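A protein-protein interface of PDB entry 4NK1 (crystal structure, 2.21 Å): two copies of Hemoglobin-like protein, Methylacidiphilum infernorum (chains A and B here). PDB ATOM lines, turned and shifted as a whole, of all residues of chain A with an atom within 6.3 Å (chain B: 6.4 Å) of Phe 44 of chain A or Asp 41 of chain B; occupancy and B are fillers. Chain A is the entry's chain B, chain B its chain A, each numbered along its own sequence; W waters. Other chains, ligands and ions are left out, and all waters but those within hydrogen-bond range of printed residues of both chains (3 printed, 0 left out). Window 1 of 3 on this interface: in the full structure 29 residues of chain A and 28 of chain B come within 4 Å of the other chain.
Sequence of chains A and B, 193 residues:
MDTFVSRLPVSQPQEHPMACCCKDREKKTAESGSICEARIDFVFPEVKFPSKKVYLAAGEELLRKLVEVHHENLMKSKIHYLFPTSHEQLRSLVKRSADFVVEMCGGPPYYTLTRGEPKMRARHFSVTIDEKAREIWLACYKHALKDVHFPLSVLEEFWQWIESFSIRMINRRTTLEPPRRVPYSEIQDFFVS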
ATOM      1  N   PHE A  42      -1.834 -32.678 -18.678  1.00  0.00           N
ATOM      2  CA  PHE A  42      -0.689 -31.987 -19.249  1.00  0.00           C
ATOM      3  C   PHE A  42       0.166 -31.387 -18.132  1.00  0.00           C
ATOM      4  O   PHE A  42      -0.302 -31.213 -16.998  1.00  0.00           O
ATOM      5  CB  PHE A  42      -1.153 -30.900 -20.236  1.00  0.00           C
ATOM      6  CG  PHE A  42      -1.891 -29.772 -19.580  1.00  0.00           C
ATOM      7  CD1 PHE A  42      -3.257 -29.861 -19.354  1.00  0.00           C
ATOM      8  CD2 PHE A  42      -1.214 -28.630 -19.163  1.00  0.00           C
ATOM      9  CE1 PHE A  42      -3.943 -28.828 -18.721  1.00  0.00           C
ATOM     10  CE2 PHE A  42      -1.888 -27.598 -18.541  1.00  0.00           C
ATOM     11  CZ  PHE A  42      -3.256 -27.693 -18.319  1.00  0.00           C
ATOM     12  N   VAL A  43       1.418 -31.072 -18.455  1.00  0.00           N
ATOM     13  CA  VAL A  43       2.327 -30.452 -17.493  1.00  0.00           C
ATOM     14  C   VAL A  43       2.222 -28.925 -17.556  1.00  0.00           C
ATOM     15  O   VAL A  43       2.210 -28.343 -18.637  1.00  0.00           O
ATOM     16  CB  VAL A  43       3.784 -30.852 -17.778  1.00  0.00           C
ATOM     17  CG1 VAL A  43       4.708 -30.369 -16.660  1.00  0.00           C
ATOM     18  CG2 VAL A  43       3.897 -32.359 -17.945  1.00  0.00           C
ATOM     19  N   PHE A  44       2.113 -28.281 -16.402  1.00  0.00           N
ATOM     20  CA  PHE A  44       2.271 -26.836 -16.334  1.00  0.00           C
ATOM     21  C   PHE A  44       3.772 -26.559 -16.372  1.00  0.00           C
ATOM     22  O   PHE A  44       4.483 -26.898 -15.428  1.00  0.00           O
ATOM     23  CB  PHE A  44       1.647 -26.294 -15.047  1.00  0.00           C
ATOM     24  CG  PHE A  44       0.165 -26.532 -14.956  1.00  0.00           C
ATOM     25  CD1 PHE A  44      -0.734 -25.576 -15.407  1.00  0.00           C
ATOM     26  CD2 PHE A  44      -0.335 -27.729 -14.452  1.00  0.00           C
ATOM     27  CE1 PHE A  44      -2.106 -25.791 -15.333  1.00  0.00           C
ATOM     28  CE2 PHE A  44      -1.706 -27.952 -14.382  1.00  0.00           C
ATOM     29  CZ  PHE A  44      -2.593 -26.973 -14.826  1.00  0.00           C
ATOM     30  N   PRO A  45       4.258 -25.970 -17.480  1.00  0.00           N
ATOM     31  CA  PRO A  45       5.691 -25.770 -17.744  1.00  0.00           C
ATOM     32  C   PRO A  45       6.324 -24.858 -16.708  1.00  0.00           C
ATOM     33  O   PRO A  45       5.603 -24.098 -16.042  1.00  0.00           O
ATOM     34  CB  PRO A  45       5.706 -25.051 -19.103  1.00  0.00           C
ATOM     35  CG  PRO A  45       4.387 -25.331 -19.718  1.00  0.00           C
ATOM     36  CD  PRO A  45       3.420 -25.442 -18.570  1.00  0.00           C
ATOM     37  N   GLU A  46       7.646 -24.927 -16.553  1.00  0.00           N
ATOM     38  CA  GLU A  46       8.299 -24.001 -15.636  1.00  0.00           C
ATOM     39  C   GLU A  46       8.110 -22.578 -16.151  1.00  0.00           C
ATOM     40  O   GLU A  46       8.113 -22.341 -17.362  1.00  0.00           O
ATOM     41  CB  GLU A  46       9.783 -24.324 -15.447  1.00  0.00           C
ATOM     42  CG  GLU A  46      10.652 -24.149 -16.677  1.00  0.00           C
ATOM     43  CD  GLU A  46      12.148 -24.129 -16.329  1.00  0.00           C
ATOM     44  OE1 GLU A  46      12.945 -23.594 -17.135  1.00  0.00           O
ATOM     45  OE2 GLU A  46      12.525 -24.653 -15.253  1.00  0.00           O
ATOM     46  N   VAL A  47       7.879 -21.643 -15.242  1.00  0.00           N
ATOM     47  CA  VAL A  47       7.785 -20.258 -15.651  1.00  0.00           C
ATOM     48  C   VAL A  47       8.921 -19.416 -15.061  1.00  0.00           C
ATOM     49  O   VAL A  47       9.181 -19.453 -13.850  1.00  0.00           O
ATOM     50  CB  VAL A  47       6.369 -19.646 -15.425  1.00  0.00           C
ATOM     51  CG1 VAL A  47       5.383 -20.684 -14.899  1.00  0.00           C
ATOM     52  CG2 VAL A  47       6.417 -18.420 -14.541  1.00  0.00           C
ATOM     53  N   ARG A 121      -3.671 -18.651 -10.045  1.00  0.00           N
ATOM     54  CA  ARG A 121      -4.543 -19.743 -10.483  1.00  0.00           C
ATOM     55  C   ARG A 121      -5.842 -19.747  -9.680  1.00  0.00           C
ATOM     56  O   ARG A 121      -6.928 -19.710 -10.258  1.00  0.00           O
ATOM     57  CB  ARG A 121      -3.847 -21.112 -10.394  1.00  0.00           C
ATOM     58  CG  ARG A 121      -4.762 -22.275 -10.801  1.00  0.00           C
ATOM     59  CD  ARG A 121      -3.988 -23.552 -11.075  1.00  0.00           C
ATOM     60  NE  ARG A 121      -4.888 -24.684 -11.290  1.00  0.00           N
ATOM     61  CZ  ARG A 121      -5.479 -24.972 -12.448  1.00  0.00           C
ATOM     62  NH1 ARG A 121      -5.274 -24.201 -13.518  1.00  0.00           N
ATOM     63  NH2 ARG A 121      -6.290 -26.025 -12.530  1.00  0.00           N
ATOM     64  N   SER A 164       4.088 -18.768 -20.560  1.00  0.00           N
ATOM     65  CA  SER A 164       4.134 -19.960 -19.728  1.00  0.00           C
ATOM     66  C   SER A 164       3.224 -19.824 -18.505  1.00  0.00           C
ATOM     67  O   SER A 164       2.487 -20.746 -18.171  1.00  0.00           O
ATOM     68  CB  SER A 164       5.578 -20.237 -19.297  1.00  0.00           C
ATOM     69  OG  SER A 164       5.640 -21.369 -18.447  1.00  0.00           O
ATOM     70  N   ILE A 167      -0.644 -20.507 -18.799  1.00  0.00           N
ATOM     71  CA  ILE A 167      -1.093 -21.895 -18.906  1.00  0.00           C
ATOM     72  C   ILE A 167      -1.692 -22.334 -17.578  1.00  0.00           C
ATOM     73  O   ILE A 167      -2.591 -23.175 -17.525  1.00  0.00           O
ATOM     74  CB  ILE A 167       0.080 -22.828 -19.288  1.00  0.00           C
ATOM     75  CG1 ILE A 167       0.543 -22.540 -20.717  1.00  0.00           C
ATOM     76  CG2 ILE A 167      -0.306 -24.300 -19.160  1.00  0.00           C
ATOM     77  CD1 ILE A 167       1.972 -22.971 -21.000  1.00  0.00           C
ATOM     78  N   ARG A 168      -1.206 -21.734 -16.499  1.00  0.00           N
ATOM     79  CA  ARG A 168      -1.646 -22.111 -15.174  1.00  0.00           C
ATOM     80  C   ARG A 168      -2.999 -21.549 -14.772  1.00  0.00           C
ATOM     81  O   ARG A 168      -3.553 -21.931 -13.735  1.00  0.00           O
ATOM     82  CB  ARG A 168      -0.571 -21.733 -14.159  1.00  0.00           C
ATOM     83  CG  ARG A 168       0.692 -22.561 -14.356  1.00  0.00           C
ATOM     84  CD  ARG A 168       1.691 -22.319 -13.271  1.00  0.00           C
ATOM     85  NE  ARG A 168       2.958 -22.969 -13.579  1.00  0.00           N
ATOM     86  CZ  ARG A 168       3.762 -23.497 -12.663  1.00  0.00           C
ATOM     87  NH1 ARG A 168       3.418 -23.448 -11.384  1.00  0.00           N
ATOM     88  NH2 ARG A 168       4.901 -24.066 -13.033  1.00  0.00           N
ATOM     89  N   MET A 169      -3.547 -20.666 -15.596  1.00  0.00           N
ATOM     90  CA  MET A 169      -4.837 -20.075 -15.290  1.00  0.00           C
ATOM     91  C   MET A 169      -5.965 -20.894 -15.919  1.00  0.00           C
ATOM     92  O   MET A 169      -7.125 -20.722 -15.561  1.00  0.00           O
ATOM     93  CB  MET A 169      -4.887 -18.618 -15.773  1.00  0.00           C
ATOM     94  CG  MET A 169      -3.686 -17.779 -15.338  1.00  0.00           C
ATOM     95  SD  MET A 169      -3.397 -17.788 -13.551  1.00  0.00           S
ATOM     96  CE  MET A 169      -1.607 -17.666 -13.552  1.00  0.00           C
ATOM     97  N   ILE A 170      -5.621 -21.796 -16.841  1.00  0.00           N
ATOM     98  CA  ILE A 170      -6.615 -22.599 -17.556  1.00  0.00           C
ATOM     99  C   ILE A 170      -7.345 -23.525 -16.585  1.00  0.00           C
ATOM    100  O   ILE A 170      -6.726 -24.380 -15.932  1.00  0.00           O
ATOM    101  CB  ILE A 170      -5.974 -23.473 -18.665  1.00  0.00           C
ATOM    102  CG1 ILE A 170      -5.423 -22.611 -19.798  1.00  0.00           C
ATOM    103  CG2 ILE A 170      -6.992 -24.440 -19.236  1.00  0.00           C
ATOM    104  CD1 ILE A 170      -4.486 -23.381 -20.714  1.00  0.00           C
ATOM    105  N   CYS B  36       9.478 -20.605 -11.255  1.00  0.00           N
ATOM    106  CA  CYS B  36       8.584 -21.604 -10.683  1.00  0.00           C
ATOM    107  C   CYS B  36       8.695 -22.878 -11.507  1.00  0.00           C
ATOM    108  O   CYS B  36       8.496 -22.856 -12.724  1.00  0.00           O
ATOM    109  CB  CYS B  36       7.149 -21.093 -10.692  1.00  0.00           C
ATOM    110  SG  CYS B  36       6.934 -19.606  -9.702  1.00  0.00           S
ATOM    111  N   GLU B  37       9.014 -23.992 -10.859  1.00  0.00           N
ATOM    112  CA  GLU B  37       9.242 -25.222 -11.610  1.00  0.00           C
ATOM    113  C   GLU B  37       7.954 -25.845 -12.144  1.00  0.00           C
ATOM    114  O   GLU B  37       6.853 -25.542 -11.673  1.00  0.00           O
ATOM    115  CB  GLU B  37      10.047 -26.242 -10.797  1.00  0.00           C
ATOM    116  CG  GLU B  37      10.650 -27.365 -11.641  1.00  0.00           C
ATOM    117  CD  GLU B  37      11.204 -26.866 -12.974  1.00  0.00           C
ATOM    118  OE1 GLU B  37      10.921 -27.504 -14.018  1.00  0.00           O
ATOM    119  OE2 GLU B  37      11.931 -25.844 -12.973  1.00  0.00           O
ATOM    120  N   ALA B  38       8.111 -26.698 -13.154  1.00  0.00           N
ATOM    121  CA  ALA B  38       7.006 -27.420 -13.757  1.00  0.00           C
ATOM    122  C   ALA B  38       6.217 -28.171 -12.698  1.00  0.00           C
ATOM    123  O   ALA B  38       6.745 -28.534 -11.641  1.00  0.00           O
ATOM    124  CB  ALA B  38       7.507 -28.385 -14.827  1.00  0.00           C
ATOM    125  N   ARG B  39       4.947 -28.406 -12.991  1.00  0.00           N
ATOM    126  CA  ARG B  39       4.042 -28.965 -12.005  1.00  0.00           C
ATOM    127  C   ARG B  39       2.860 -29.619 -12.699  1.00  0.00           C
ATOM    128  O   ARG B  39       2.547 -29.315 -13.855  1.00  0.00           O
ATOM    129  CB  ARG B  39       3.555 -27.856 -11.062  1.00  0.00           C
ATOM    130  CG  ARG B  39       4.004 -28.050  -9.625  1.00  0.00           C
ATOM    131  CD  ARG B  39       3.435 -26.996  -8.676  1.00  0.00           C
ATOM    132  NE  ARG B  39       3.606 -27.390  -7.276  1.00  0.00           N
ATOM    133  CZ  ARG B  39       4.764 -27.357  -6.616  1.00  0.00           C
ATOM    134  NH1 ARG B  39       5.876 -26.945  -7.219  1.00  0.00           N
ATOM    135  NH2 ARG B  39       4.812 -27.741  -5.346  1.00  0.00           N
ATOM    136  N   ILE B  40       2.206 -30.536 -12.007  1.00  0.00           N
ATOM    137  CA  ILE B  40       0.953 -31.060 -12.516  1.00  0.00           C
ATOM    138  C   ILE B  40      -0.146 -30.655 -11.551  1.00  0.00           C
ATOM    139  O   ILE B  40       0.128 -30.352 -10.390  1.00  0.00           O
ATOM    140  CB  ILE B  40       0.995 -32.586 -12.705  1.00  0.00           C
ATOM    141  CG1 ILE B  40       1.476 -33.265 -11.432  1.00  0.00           C
ATOM    142  CG2 ILE B  40       1.911 -32.958 -13.867  1.00  0.00           C
ATOM    143  CD1 ILE B  40       1.602 -34.769 -11.570  1.00  0.00           C
ATOM    144  N   ASP B  41      -1.380 -30.619 -12.035  1.00  0.00           N
ATOM    145  CA  ASP B  41      -2.505 -30.282 -11.182  1.00  0.00           C
ATOM    146  C   ASP B  41      -2.827 -31.499 -10.321  1.00  0.00           C
ATOM    147  O   ASP B  41      -2.783 -31.430  -9.088  1.00  0.00           O
ATOM    148  CB  ASP B  41      -3.700 -29.908 -12.044  1.00  0.00           C
ATOM    149  CG  ASP B  41      -4.814 -29.280 -11.250  1.00  0.00           C
ATOM    150  OD1 ASP B  41      -4.643 -29.075 -10.024  1.00  0.00           O
ATOM    151  OD2 ASP B  41      -5.862 -28.975 -11.857  1.00  0.00           O
ATOM    152  N   PHE B  42      -3.141 -32.609 -10.983  1.00  0.00           N
ATOM    153  CA  PHE B  42      -3.343 -33.889 -10.305  1.00  0.00           C
ATOM    154  C   PHE B  42      -3.205 -35.047 -11.289  1.00  0.00           C
ATOM    155  O   PHE B  42      -3.311 -34.863 -12.513  1.00  0.00           O
ATOM    156  CB  PHE B  42      -4.712 -33.942  -9.617  1.00  0.00           C
ATOM    157  CG  PHE B  42      -5.864 -33.901 -10.569  1.00  0.00           C
ATOM    158  CD1 PHE B  42      -6.472 -35.070 -10.990  1.00  0.00           C
ATOM    159  CD2 PHE B  42      -6.332 -32.699 -11.056  1.00  0.00           C
ATOM    160  CE1 PHE B  42      -7.541 -35.035 -11.876  1.00  0.00           C
ATOM    161  CE2 PHE B  42      -7.399 -32.661 -11.952  1.00  0.00           C
ATOM    162  CZ  PHE B  42      -8.002 -33.837 -12.358  1.00  0.00           C
ATOM    163  N   VAL B  43      -2.965 -36.239 -10.748  1.00  0.00           N
ATOM    164  CA  VAL B  43      -2.832 -37.447 -11.558  1.00  0.00           C
ATOM    165  C   VAL B  43      -4.196 -38.102 -11.780  1.00  0.00           C
ATOM    166  O   VAL B  43      -4.984 -38.219 -10.843  1.00  0.00           O
ATOM    167  CB  VAL B  43      -1.896 -38.459 -10.868  1.00  0.00           C
ATOM    168  CG1 VAL B  43      -1.667 -39.684 -11.761  1.00  0.00           C
ATOM    169  CG2 VAL B  43      -0.567 -37.794 -10.507  1.00  0.00           C
ATOM    170  N   ARG B 173     -11.902 -27.102 -13.204  1.00  0.00           N
ATOM    171  CA  ARG B 173     -11.273 -27.068 -11.889  1.00  0.00           C
ATOM    172  C   ARG B 173     -11.661 -25.813 -11.127  1.00  0.00           C
ATOM    173  O   ARG B 173     -11.699 -24.709 -11.691  1.00  0.00           O
ATOM    174  CB  ARG B 173      -9.751 -27.157 -12.013  1.00  0.00           C
ATOM    175  CG  ARG B 173      -9.283 -28.493 -12.549  1.00  0.00           C
ATOM    176  CD  ARG B 173      -9.354 -29.543 -11.465  1.00  0.00           C
ATOM    177  NE  ARG B 173      -8.128 -29.573 -10.680  1.00  0.00           N
ATOM    178  CZ  ARG B 173      -8.071 -29.855  -9.379  1.00  0.00           C
ATOM    179  NH1 ARG B 173      -9.185 -30.129  -8.705  1.00  0.00           N
ATOM    180  NH2 ARG B 173      -6.901 -29.859  -8.749  1.00  0.00           N
ATOM    181  N   THR B 175     -10.600 -25.628  -7.592  1.00  0.00           N
ATOM    182  CA  THR B 175      -9.812 -25.699  -6.374  1.00  0.00           C
ATOM    183  C   THR B 175      -8.445 -26.253  -6.714  1.00  0.00           C
ATOM    184  O   THR B 175      -8.299 -26.970  -7.716  1.00  0.00           O
ATOM    185  CB  THR B 175     -10.490 -26.639  -5.330  1.00  0.00           C
ATOM    186  OG1 THR B 175      -9.713 -26.681  -4.128  1.00  0.00           O
ATOM    187  CG2 THR B 175     -10.620 -28.067  -5.874  1.00  0.00           C
ATOM    188  N   LEU B 176      -7.447 -25.935  -5.889  1.00  0.00           N
ATOM    189  CA  LEU B 176      -6.111 -26.506  -6.059  1.00  0.00           C
ATOM    190  C   LEU B 176      -6.044 -27.931  -5.498  1.00  0.00           C
ATOM    191  O   LEU B 176      -5.184 -28.726  -5.894  1.00  0.00           O
ATOM    192  CB  LEU B 176      -5.065 -25.634  -5.364  1.00  0.00           C
ATOM    193  CG  LEU B 176      -4.864 -24.216  -5.883  1.00  0.00           C
ATOM    194  CD1 LEU B 176      -3.839 -23.493  -5.007  1.00  0.00           C
ATOM    195  CD2 LEU B 176      -4.410 -24.241  -7.339  1.00  0.00           C
ATOM    196  N   GLU B 177      -6.947 -28.247  -4.571  1.00  0.00           N
ATOM    197  CA  GLU B 177      -7.038 -29.587  -3.987  1.00  0.00           C
ATOM    198  C   GLU B 177      -7.334 -30.658  -5.044  1.00  0.00           C
ATOM    199  O   GLU B 177      -8.050 -30.391  -6.015  1.00  0.00           O
ATOM    200  CB  GLU B 177      -8.146 -29.614  -2.931  1.00  0.00           C
ATOM    201  CG  GLU B 177      -7.903 -28.697  -1.749  1.00  0.00           C
ATOM    202  CD  GLU B 177      -6.720 -29.139  -0.898  1.00  0.00           C
ATOM    203  OE1 GLU B 177      -5.561 -28.872  -1.283  1.00  0.00           O
ATOM    204  OE2 GLU B 177      -6.945 -29.756   0.164  1.00  0.00           O
ATOM    205  N   PRO B 178      -6.788 -31.879  -4.855  1.00  0.00           N
ATOM    206  CA  PRO B 178      -7.088 -32.978  -5.781  1.00  0.00           C
ATOM    207  C   PRO B 178      -8.526 -33.447  -5.595  1.00  0.00           C
ATOM    208  O   PRO B 178      -9.121 -33.142  -4.562  1.00  0.00           O
ATOM    209  CB  PRO B 178      -6.131 -34.100  -5.349  1.00  0.00           C
ATOM    210  CG  PRO B 178      -5.241 -33.523  -4.271  1.00  0.00           C
ATOM    211  CD  PRO B 178      -5.950 -32.316  -3.723  1.00  0.00           C
HETATM  212  O   HOH W   1      -1.767 -31.867 -14.507  1.00  0.00           O
HETATM  213  O   HOH W   2      -6.255 -26.919  -9.649  1.00  0.00           O
HETATM  214  O   HOH W   3       5.637 -24.242  -9.428  1.00  0.00           O
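Of chain B, only Ala 38 (3.1 Å), Arg 39 (2.8 Å) and Asp 41 (3.6 Å) come within 4 Å of Phe 44 of chain A.
Of the printed residues of chain B, Glu 46 of chain A touches Cys 36, Glu 37 and Ala 38.
Of the printed residues of chain B, Val 47 of chain A touches Cys 36 (2.9 Å).
Printed residues of chain B within 4 Å of Arg 168 of chain A: Cys 36 (3.8 Å) and Glu 37 (2.8 Å).
Of the printed residues of chain A, Ala 38 of chain B touches Val 43 (3.9 Å), Phe 44 (3.1 Å), Pro 45 (3.97 Å) and Glu 46 (3.7 Å).
Of the printed residues of chain A, Arg 39 of chain B touches Val 43 (3.7 Å) and Phe 44 (2.8 Å).
Asp 41 of chain B touches two residues of chain A.
The nearest residue of chain B that does not touch Phe 44 of chain A is Ile 40 of chain B (4.1 Å).
The nearest residue of chain A that does not touch Asp 41 of chain B is Phe 42 of chain A (5.1 Å).
The nearest printed residue of chain B that does not touch Val 43 of chain A is Ile 40 of chain B (4.4 Å).
The guanidinium group of Arg 121 of chain A is in hydrogen-bond range of the backbone carbonyl oxygen of Arg 168 of chain A, 2.9 Å away.
N of Arg 121 of chain A is in hydrogen-bond range of SD of Met 169 of chain A (3.6 Å).
The guanidinium group (NH1) of Arg 121 of chain A sits at hydrogen-bond distance from the backbone carbonyl oxygen (O) of Ile 170 of chain A, at 2.8 Å.
NH1 of Arg 173 of chain B sits at hydrogen-bond distance from O of Glu 177 of chain B.
The backbone carbonyl oxygen (O) of Glu 46 of chain A is in hydrogen-bond range of the side-chain hydroxyl (OG) of Ser 164 of chain A.
The guanidinium group (NH2) of Arg 173 of chain B sits close to the backbone carbonyl oxygen (O) of Thr 175 of chain B (3.4 Å).
Among the printed residues, pairs that only touch across the chains: Phe 44 of chain A with Ala 38 of chain B (3.1 Å), Glu 46 of chain A with Cys 36 of chain B (3.1 Å), Phe 44 of chain A with Asp 41 of chain B (3.6 Å), Glu 46 of chain A with Ala 38 of chain B (3.7 Å), Arg 121 of chain A with Arg 173 of chain B (3.7 Å), Val 43 of chain A with Arg 39 of chain B (3.7 Å), Arg 168 of chain A with Cys 36 of chain B (3.8 Å), Arg 121 of chain A with Leu 176 of chain B (3.8 Å), Val 43 of chain A with Ala 38 of chain B (3.9 Å) and Pro 45 of chain A with Ala 38 of chain B (3.97 Å).
Water W2 lies within hydrogen-bond range of the side-chain carboxylate of Asp 41 of chain B (2.7 Å), the backbone carbonyl oxygen of Thr 175 of chain B (2.8 Å), the guanidinium group of Arg 121 of chain A (3.0 Å) and the guanidinium group of Arg 173 of chain B (3.1 Å).
Water W1 lies within hydrogen-bond range of N of Asp 41 of chain B and O of Phe 42 of chain A.
Water W3 lies within hydrogen-bond range of O of Glu 37 of chain B (2.9 Å), NH1 of Arg 168 of chain A (3.1 Å) and NH1 of Arg 39 of chain B (3.5 Å).
The backbone NH (N) of Cys 36 of chain B lies within hydrogen-bond range of the backbone carbonyl oxygen (O) of Val 47 of chain A, at 2.9 Å.
N of Phe 44 of chain A lies within hydrogen-bond range of O of Arg 39 of chain B.
O of Glu 37 of chain B lies within hydrogen-bond range of NH2 of Arg 168 of chain A, at 2.8 Å.
OD2 of Asp 41 of chain B lies within salt-bridge range of NH2 of Arg 121 of chain A.
The side-chain carboxylate of Glu 37 of chain B sits close to the side-chain carboxylate of Glu 46 of chain A (2.6 Å).
Printed residues of chain B that touch a printed residue of chain A: Cys 36, Glu 37, Ala 38, Arg 39, Asp 41, Arg 173 and Leu 176.
Hydrophobic or aromatic side chains of chain B that line the printed part of chain A: Ala 38 and Leu 176.
Of the 12 printed residues of chain A, 7 touch a printed residue of chain B.
Printed residues of chain A that touch a printed residue of chain B: Val 43, Phe 44, Pro 45, Glu 46, Val 47, Arg 121 and Arg 168.
Hydrophobic or aromatic side chains of chain A that line the printed part of chain B: Val 43 and Phe 44.
Among the printed residues, 15 pairs touch across the chains.
2 positions are printed for both chains.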
